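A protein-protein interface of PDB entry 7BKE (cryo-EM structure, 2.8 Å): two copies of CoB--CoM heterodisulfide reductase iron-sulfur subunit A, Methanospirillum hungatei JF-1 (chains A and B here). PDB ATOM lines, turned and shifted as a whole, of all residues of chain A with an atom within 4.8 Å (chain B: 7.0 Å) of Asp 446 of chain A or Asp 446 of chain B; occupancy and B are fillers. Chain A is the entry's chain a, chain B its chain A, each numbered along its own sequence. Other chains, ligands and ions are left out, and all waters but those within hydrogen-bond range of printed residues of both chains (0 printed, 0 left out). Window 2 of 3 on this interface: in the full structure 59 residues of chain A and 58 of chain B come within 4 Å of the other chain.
The side-chain sulfur (SG) of Cys 421 of chain A sits close to the backbone NH (N) of Arg 448 of chain A, at 3.3 Å. The backbone carbonyl oxygen (O) of Asp 446 of chain A lies close to the side-chain sulfur (SG) of Cys 421 of chain A, at 3.6 Å. The guanidinium group (NH2) of Arg 406 of chain A is in salt-bridge range of the side-chain carboxylate (OD2) of Asp 446 of chain A (3.4 Å). SG of Cys 421 of chain B sits close to O of Asp 446 of chain B, 3.6 Å away. NH1 of Arg 406 of chain A lies within hydrogen-bond range of O of Met 445 of chain A, 2.8 Å away. NH2 of Arg 406 of chain B lies within salt-bridge range of OD2 of Asp 446 of chain B, at 3.4 Å.
The backbone carbonyl oxygen (O) of Ile 447 of chain B is in hydrogen-bond range of the guanidinium group (NE) of Arg 448 of chain A (3.2 Å). OD1 of Asp 446 of chain B sits at hydrogen-bond distance from N of Ile 447 of chain A (3.2 Å). The guanidinium group (NE) of Arg 448 of chain B sits at hydrogen-bond distance from the backbone carbonyl oxygen (O) of Ile 447 of chain A (3.2 Å). The backbone carbonyl oxygen of Ser 449 of chain B lies within hydrogen-bond range of the guanidinium group of Arg 448 of chain A. The side-chain carboxylate of Glu 455 of chain B is in salt-bridge range of the guanidinium group of Arg 448 of chain A. OE2 of Glu 455 of chain B is in salt-bridge range of NE of Arg 406 of chain A, 3.3 Å away. The side-chain carboxylate (OD1) of Asp 446 of chain A lies within hydrogen-bond range of the backbone NH (N) of Ile 447 of chain B (3.2 Å).
Printed residues of chain A that touch a printed residue of chain B: Arg 406, Asp 446, Ile 447 and Arg 448. Among the printed residues, Asp or Glu carboxylates within 4 Å of a Lys or Arg side-chain nitrogen of the other chain: Arg 406 of chain A with Glu 455 of chain B (3.3 Å) and Arg 448 of chain A with Glu 455 of chain B (2.9 Å).
Asp 446 of chain B touches its own counterpart, Asp 446 of chain A. Asp 446 of chain A touches Ile 447 of chain B, and with the chains exchanged Ile 447 of chain A touches Asp 446 of chain B. Ile 447 of chain A touches Arg 448 of chain B, and with the chains exchanged Arg 448 of chain A touches Ile 447 of chain B. Arg 448 of chain B touches its own counterpart, Arg 448 of chain A. Of the 9 pairs that touch across the chains among the printed residues, 6 have their exchanged pair printed and touching as well.
OD1 of Asp 446 of chain B touches CA of Asp 446 of chain A, at 3.4 Å. CG of Arg 448 of chain A touches CG of Arg 448 of chain B, 3.9 Å away.
Asp 446 of chain A touches just these residues of chain B: Asp 446 (3.4 Å) and Ile 447 (3.2 Å). Of chain A, only Asp 446 and Ile 447 come within 4 Å of Asp 446 of chain B. Printed residues of chain B within 4 Å of Ile 447 of chain A: Asp 446 and Arg 448. Printed residues of chain B within 4 Å of Arg 448 of chain A: Ile 447 (3.2 Å), Arg 448 (3.9 Å), Ser 449 (2.9 Å) and Glu 455 (2.9 Å). Of the printed residues of chain A, Arg 448 of chain B touches Ile 447 and Arg 448. Of the printed residues of chain A, Glu 455 of chain B touches Arg 406 (3.3 Å) and Arg 448 (2.9 Å). Tyr 458 of chain B touches none of the printed residues of chain A. The nearest residue of chain B that does not touch Asp 446 of chain A is Tyr 444 of chain B (4.4 Å).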
ATOM      1  N   ARG A 406       2.677 -11.316 -18.836  1.00  0.00           N
ATOM      2  CA  ARG A 406       4.079 -11.798 -18.810  1.00  0.00           C
ATOM      3  C   ARG A 406       4.916 -10.527 -18.910  1.00  0.00           C
ATOM      4  O   ARG A 406       5.928 -10.570 -19.609  1.00  0.00           O
ATOM      5  CB  ARG A 406       4.207 -12.851 -19.907  1.00  0.00           C
ATOM      6  CG  ARG A 406       2.992 -13.754 -20.047  1.00  0.00           C
ATOM      7  CD  ARG A 406       3.129 -14.651 -21.251  1.00  0.00           C
ATOM      8  NE  ARG A 406       4.503 -15.087 -21.391  1.00  0.00           N
ATOM      9  CZ  ARG A 406       5.033 -15.574 -22.502  1.00  0.00           C
ATOM     10  NH1 ARG A 406       4.295 -15.691 -23.590  1.00  0.00           N
ATOM     11  NH2 ARG A 406       6.294 -15.950 -22.518  1.00  0.00           N
ATOM     12  N   CYS A 421      -4.739 -16.861 -25.570  1.00  0.00           N
ATOM     13  CA  CYS A 421      -4.207 -17.411 -26.840  1.00  0.00           C
ATOM     14  C   CYS A 421      -5.361 -18.153 -27.501  1.00  0.00           C
ATOM     15  O   CYS A 421      -5.542 -18.000 -28.681  1.00  0.00           O
ATOM     16  CB  CYS A 421      -3.063 -18.400 -26.656  1.00  0.00           C
ATOM     17  SG  CYS A 421      -1.411 -17.723 -26.375  1.00  0.00           S
ATOM     18  N   TYR A 444       2.069 -12.880 -31.934  1.00  0.00           N
ATOM     19  CA  TYR A 444       2.058 -13.772 -30.799  1.00  0.00           C
ATOM     20  C   TYR A 444       3.453 -13.960 -30.241  1.00  0.00           C
ATOM     21  O   TYR A 444       4.451 -13.490 -30.779  1.00  0.00           O
ATOM     22  CB  TYR A 444       1.449 -15.132 -31.170  1.00  0.00           C
ATOM     23  CG  TYR A 444       2.387 -16.056 -31.896  1.00  0.00           C
ATOM     24  CD1 TYR A 444       3.192 -16.936 -31.204  1.00  0.00           C
ATOM     25  CD2 TYR A 444       2.455 -16.062 -33.276  1.00  0.00           C
ATOM     26  CE1 TYR A 444       4.043 -17.773 -31.853  1.00  0.00           C
ATOM     27  CE2 TYR A 444       3.309 -16.900 -33.934  1.00  0.00           C
ATOM     28  CZ  TYR A 444       4.098 -17.757 -33.216  1.00  0.00           C
ATOM     29  OH  TYR A 444       4.958 -18.610 -33.861  1.00  0.00           O
ATOM     30  N   MET A 445       3.601 -14.523 -29.076  1.00  0.00           N
ATOM     31  CA  MET A 445       4.916 -14.712 -28.430  1.00  0.00           C
ATOM     32  C   MET A 445       4.740 -15.945 -27.567  1.00  0.00           C
ATOM     33  O   MET A 445       4.549 -15.735 -26.360  1.00  0.00           O
ATOM     34  CB  MET A 445       5.123 -13.510 -27.510  1.00  0.00           C
ATOM     35  CG  MET A 445       6.393 -13.469 -26.703  1.00  0.00           C
ATOM     36  SD  MET A 445       6.263 -11.983 -25.688  1.00  0.00           S
ATOM     37  CE  MET A 445       5.198 -12.519 -24.354  1.00  0.00           C
ATOM     38  N   ASP A 446       4.675 -17.135 -28.134  1.00  0.00           N
ATOM     39  CA  ASP A 446       4.332 -18.399 -27.407  1.00  0.00           C
ATOM     40  C   ASP A 446       2.845 -18.698 -27.479  1.00  0.00           C
ATOM     41  O   ASP A 446       2.162 -18.314 -26.556  1.00  0.00           O
ATOM     42  CB  ASP A 446       4.870 -18.583 -25.984  1.00  0.00           C
ATOM     43  CG  ASP A 446       6.378 -18.625 -25.852  1.00  0.00           C
ATOM     44  OD1 ASP A 446       6.972 -19.650 -26.211  1.00  0.00           O
ATOM     45  OD2 ASP A 446       6.939 -17.635 -25.359  1.00  0.00           O
ATOM     46  N   ILE A 447       2.362 -19.265 -28.577  1.00  0.00           N
ATOM     47  CA  ILE A 447       1.007 -19.807 -28.632  1.00  0.00           C
ATOM     48  C   ILE A 447       0.855 -20.897 -27.583  1.00  0.00           C
ATOM     49  O   ILE A 447       1.648 -21.841 -27.532  1.00  0.00           O
ATOM     50  CB  ILE A 447       0.690 -20.355 -30.034  1.00  0.00           C
ATOM     51  CG1 ILE A 447       0.683 -19.240 -31.077  1.00  0.00           C
ATOM     52  CG2 ILE A 447      -0.652 -21.055 -30.023  1.00  0.00           C
ATOM     53  CD1 ILE A 447      -0.531 -18.376 -31.041  1.00  0.00           C
ATOM     54  N   ARG A 448      -0.171 -20.771 -26.727  1.00  0.00           N
ATOM     55  CA  ARG A 448      -0.353 -21.660 -25.544  1.00  0.00           C
ATOM     56  C   ARG A 448      -1.673 -22.431 -25.659  1.00  0.00           C
ATOM     57  O   ARG A 448      -2.640 -22.025 -25.048  1.00  0.00           O
ATOM     58  CB  ARG A 448      -0.159 -20.860 -24.245  1.00  0.00           C
ATOM     59  CG  ARG A 448       1.295 -20.570 -23.910  1.00  0.00           C
ATOM     60  CD  ARG A 448       1.511 -19.791 -22.633  1.00  0.00           C
ATOM     61  NE  ARG A 448       2.935 -19.586 -22.456  1.00  0.00           N
ATOM     62  CZ  ARG A 448       3.491 -18.927 -21.453  1.00  0.00           C
ATOM     63  NH1 ARG A 448       4.804 -18.816 -21.387  1.00  0.00           N
ATOM     64  NH2 ARG A 448       2.738 -18.376 -20.527  1.00  0.00           N
ATOM     65  N   LEU B 401      12.204 -30.994 -25.390  1.00  0.00           N
ATOM     66  CA  LEU B 401      10.785 -30.763 -25.096  1.00  0.00           C
ATOM     67  C   LEU B 401       9.961 -31.133 -26.318  1.00  0.00           C
ATOM     68  O   LEU B 401      10.539 -31.158 -27.402  1.00  0.00           O
ATOM     69  CB  LEU B 401      10.599 -29.289 -24.733  1.00  0.00           C
ATOM     70  CG  LEU B 401      10.798 -28.920 -23.266  1.00  0.00           C
ATOM     71  CD1 LEU B 401      12.270 -28.927 -22.899  1.00  0.00           C
ATOM     72  CD2 LEU B 401      10.201 -27.554 -22.987  1.00  0.00           C
ATOM     73  N   CYS B 402       8.725 -31.557 -26.126  1.00  0.00           N
ATOM     74  CA  CYS B 402       7.783 -31.843 -27.231  1.00  0.00           C
ATOM     75  C   CYS B 402       8.171 -33.181 -27.853  1.00  0.00           C
ATOM     76  O   CYS B 402       7.841 -33.385 -28.994  1.00  0.00           O
ATOM     77  CB  CYS B 402       7.655 -30.696 -28.216  1.00  0.00           C
ATOM     78  SG  CYS B 402       6.577 -29.333 -27.724  1.00  0.00           S
ATOM     79  N   ARG B 406       2.578 -32.823 -30.337  1.00  0.00           N
ATOM     80  CA  ARG B 406       2.222 -31.812 -31.361  1.00  0.00           C
ATOM     81  C   ARG B 406       2.838 -32.346 -32.650  1.00  0.00           C
ATOM     82  O   ARG B 406       3.355 -31.529 -33.412  1.00  0.00           O
ATOM     83  CB  ARG B 406       2.684 -30.458 -30.829  1.00  0.00           C
ATOM     84  CG  ARG B 406       2.481 -30.274 -29.335  1.00  0.00           C
ATOM     85  CD  ARG B 406       3.112 -28.987 -28.865  1.00  0.00           C
ATOM     86  NE  ARG B 406       2.924 -27.950 -29.858  1.00  0.00           N
ATOM     87  CZ  ARG B 406       3.634 -26.837 -29.931  1.00  0.00           C
ATOM     88  NH1 ARG B 406       4.593 -26.605 -29.056  1.00  0.00           N
ATOM     89  NH2 ARG B 406       3.374 -25.953 -30.872  1.00  0.00           N
ATOM     90  N   CYS B 421       6.495 -29.047 -20.262  1.00  0.00           N
ATOM     91  CA  CYS B 421       7.313 -27.811 -20.284  1.00  0.00           C
ATOM     92  C   CYS B 421       7.639 -27.488 -18.832  1.00  0.00           C
ATOM     93  O   CYS B 421       8.763 -27.164 -18.554  1.00  0.00           O
ATOM     94  CB  CYS B 421       6.601 -26.603 -20.880  1.00  0.00           C
ATOM     95  SG  CYS B 421       6.541 -26.476 -22.681  1.00  0.00           S
ATOM     96  N   TYR B 444      13.430 -26.065 -27.024  1.00  0.00           N
ATOM     97  CA  TYR B 444      12.013 -25.897 -26.796  1.00  0.00           C
ATOM     98  C   TYR B 444      11.326 -25.351 -28.030  1.00  0.00           C
ATOM     99  O   TYR B 444      11.941 -25.003 -29.034  1.00  0.00           O
ATOM    100  CB  TYR B 444      11.753 -24.978 -25.595  1.00  0.00           C
ATOM    101  CG  TYR B 444      11.887 -23.509 -25.893  1.00  0.00           C
ATOM    102  CD1 TYR B 444      10.802 -22.771 -26.320  1.00  0.00           C
ATOM    103  CD2 TYR B 444      13.094 -22.858 -25.732  1.00  0.00           C
ATOM    104  CE1 TYR B 444      10.917 -21.445 -26.594  1.00  0.00           C
ATOM    105  CE2 TYR B 444      13.214 -21.525 -26.006  1.00  0.00           C
ATOM    106  CZ  TYR B 444      12.121 -20.824 -26.432  1.00  0.00           C
ATOM    107  OH  TYR B 444      12.224 -19.483 -26.707  1.00  0.00           O
ATOM    108  N   MET B 445      10.024 -25.373 -28.095  1.00  0.00           N
ATOM    109  CA  MET B 445       9.265 -24.902 -29.272  1.00  0.00           C
ATOM    110  C   MET B 445       7.943 -24.428 -28.704  1.00  0.00           C
ATOM    111  O   MET B 445       6.993 -25.217 -28.820  1.00  0.00           O
ATOM    112  CB  MET B 445       9.001 -26.133 -30.135  1.00  0.00           C
ATOM    113  CG  MET B 445       8.211 -25.933 -31.401  1.00  0.00           C
ATOM    114  SD  MET B 445       8.021 -27.579 -32.111  1.00  0.00           S
ATOM    115  CE  MET B 445       6.679 -28.263 -31.144  1.00  0.00           C
ATOM    116  N   ASP B 446       7.891 -23.297 -28.024  1.00  0.00           N
ATOM    117  CA  ASP B 446       6.687 -22.817 -27.275  1.00  0.00           C
ATOM    118  C   ASP B 446       6.727 -23.250 -25.820  1.00  0.00           C
ATOM    119  O   ASP B 446       6.145 -24.275 -25.536  1.00  0.00           O
ATOM    120  CB  ASP B 446       5.305 -23.060 -27.893  1.00  0.00           C
ATOM    121  CG  ASP B 446       5.052 -22.384 -29.224  1.00  0.00           C
ATOM    122  OD1 ASP B 446       4.843 -21.163 -29.233  1.00  0.00           O
ATOM    123  OD2 ASP B 446       5.038 -23.097 -30.238  1.00  0.00           O
ATOM    124  N   ILE B 447       7.466 -22.554 -24.969  1.00  0.00           N
ATOM    125  CA  ILE B 447       7.367 -22.748 -23.524  1.00  0.00           C
ATOM    126  C   ILE B 447       5.946 -22.455 -23.070  1.00  0.00           C
ATOM    127  O   ILE B 447       5.397 -21.387 -23.356  1.00  0.00           O
ATOM    128  CB  ILE B 447       8.369 -21.853 -22.777  1.00  0.00           C
ATOM    129  CG1 ILE B 447       9.810 -22.240 -23.103  1.00  0.00           C
ATOM    130  CG2 ILE B 447       8.137 -21.950 -21.284  1.00  0.00           C
ATOM    131  CD1 ILE B 447      10.275 -23.483 -22.424  1.00  0.00           C
ATOM    132  N   ARG B 448       5.330 -23.412 -22.358  1.00  0.00           N
ATOM    133  CA  ARG B 448       3.887 -23.347 -21.989  1.00  0.00           C
ATOM    134  C   ARG B 448       3.731 -23.323 -20.464  1.00  0.00           C
ATOM    135  O   ARG B 448       3.458 -24.357 -19.891  1.00  0.00           O
ATOM    136  CB  ARG B 448       3.102 -24.446 -22.724  1.00  0.00           C
ATOM    137  CG  ARG B 448       2.829 -24.139 -24.187  1.00  0.00           C
ATOM    138  CD  ARG B 448       2.052 -25.203 -24.928  1.00  0.00           C
ATOM    139  NE  ARG B 448       1.882 -24.773 -26.302  1.00  0.00           N
ATOM    140  CZ  ARG B 448       1.263 -25.464 -27.244  1.00  0.00           C
ATOM    141  NH1 ARG B 448       1.154 -24.966 -28.461  1.00  0.00           N
ATOM    142  NH2 ARG B 448       0.763 -26.650 -26.974  1.00  0.00           N
ATOM    143  N   SER B 449       3.960 -22.166 -19.846  1.00  0.00           N
ATOM    144  CA  SER B 449       3.832 -21.989 -18.406  1.00  0.00           C
ATOM    145  C   SER B 449       2.600 -21.120 -18.177  1.00  0.00           C
ATOM    146  O   SER B 449       2.682 -19.904 -18.031  1.00  0.00           O
ATOM    147  CB  SER B 449       5.084 -21.371 -17.834  1.00  0.00           C
ATOM    148  OG  SER B 449       5.364 -20.134 -18.450  1.00  0.00           O
ATOM    149  N   GLU B 455       4.487 -18.834 -14.822  1.00  0.00           N
ATOM    150  CA  GLU B 455       5.322 -17.854 -15.503  1.00  0.00           C
ATOM    151  C   GLU B 455       6.430 -17.358 -14.587  1.00  0.00           C
ATOM    152  O   GLU B 455       7.565 -17.146 -15.026  1.00  0.00           O
ATOM    153  CB  GLU B 455       4.465 -16.699 -16.000  1.00  0.00           C
ATOM    154  CG  GLU B 455       5.176 -15.755 -16.931  1.00  0.00           C
ATOM    155  CD  GLU B 455       5.474 -16.378 -18.275  1.00  0.00           C
ATOM    156  OE1 GLU B 455       4.691 -17.245 -18.709  1.00  0.00           O
ATOM    157  OE2 GLU B 455       6.490 -16.006 -18.894  1.00  0.00           O
ATOM    158  N   TYR B 458       9.062 -19.957 -14.558  1.00  0.00           N
ATOM    159  CA  TYR B 458       9.845 -19.851 -15.785  1.00  0.00           C
ATOM    160  C   TYR B 458      10.868 -18.724 -15.689  1.00  0.00           C
ATOM    161  O   TYR B 458      12.042 -18.888 -16.058  1.00  0.00           O
ATOM    162  CB  TYR B 458       8.877 -19.635 -16.945  1.00  0.00           C
ATOM    163  CG  TYR B 458       9.467 -19.280 -18.279  1.00  0.00           C
ATOM    164  CD1 TYR B 458      10.629 -19.875 -18.734  1.00  0.00           C
ATOM    165  CD2 TYR B 458       8.830 -18.373 -19.106  1.00  0.00           C
ATOM    166  CE1 TYR B 458      11.154 -19.554 -19.957  1.00  0.00           C
ATOM    167  CE2 TYR B 458       9.344 -18.050 -20.333  1.00  0.00           C
ATOM    168  CZ  TYR B 458      10.509 -18.642 -20.754  1.00  0.00           C
ATOM    169  OH  TYR B 458      11.024 -18.315 -21.981  1.00  0.00           O
ATOM    170  N   ARG B 470      15.347 -22.066 -28.837  1.00  0.00           N
ATOM    171  CA  ARG B 470      14.080 -22.322 -29.512  1.00  0.00           C
ATOM    172  C   ARG B 470      14.353 -23.071 -30.801  1.00  0.00           C
ATOM    173  O   ARG B 470      14.529 -22.484 -31.865  1.00  0.00           O
ATOM    174  CB  ARG B 470      13.317 -21.040 -29.787  1.00  0.00           C
ATOM    175  CG  ARG B 470      11.901 -21.324 -30.194  1.00  0.00           C
ATOM    176  CD  ARG B 470      11.268 -20.171 -30.889  1.00  0.00           C
ATOM    177  NE  ARG B 470       9.985 -20.531 -31.469  1.00  0.00           N
ATOM    178  CZ  ARG B 470       9.835 -21.176 -32.619  1.00  0.00           C
ATOM    179  NH1 ARG B 470      10.891 -21.540 -33.322  1.00  0.00           N
ATOM    180  NH2 ARG B 470       8.626 -21.455 -33.063  1.00  0.00           N
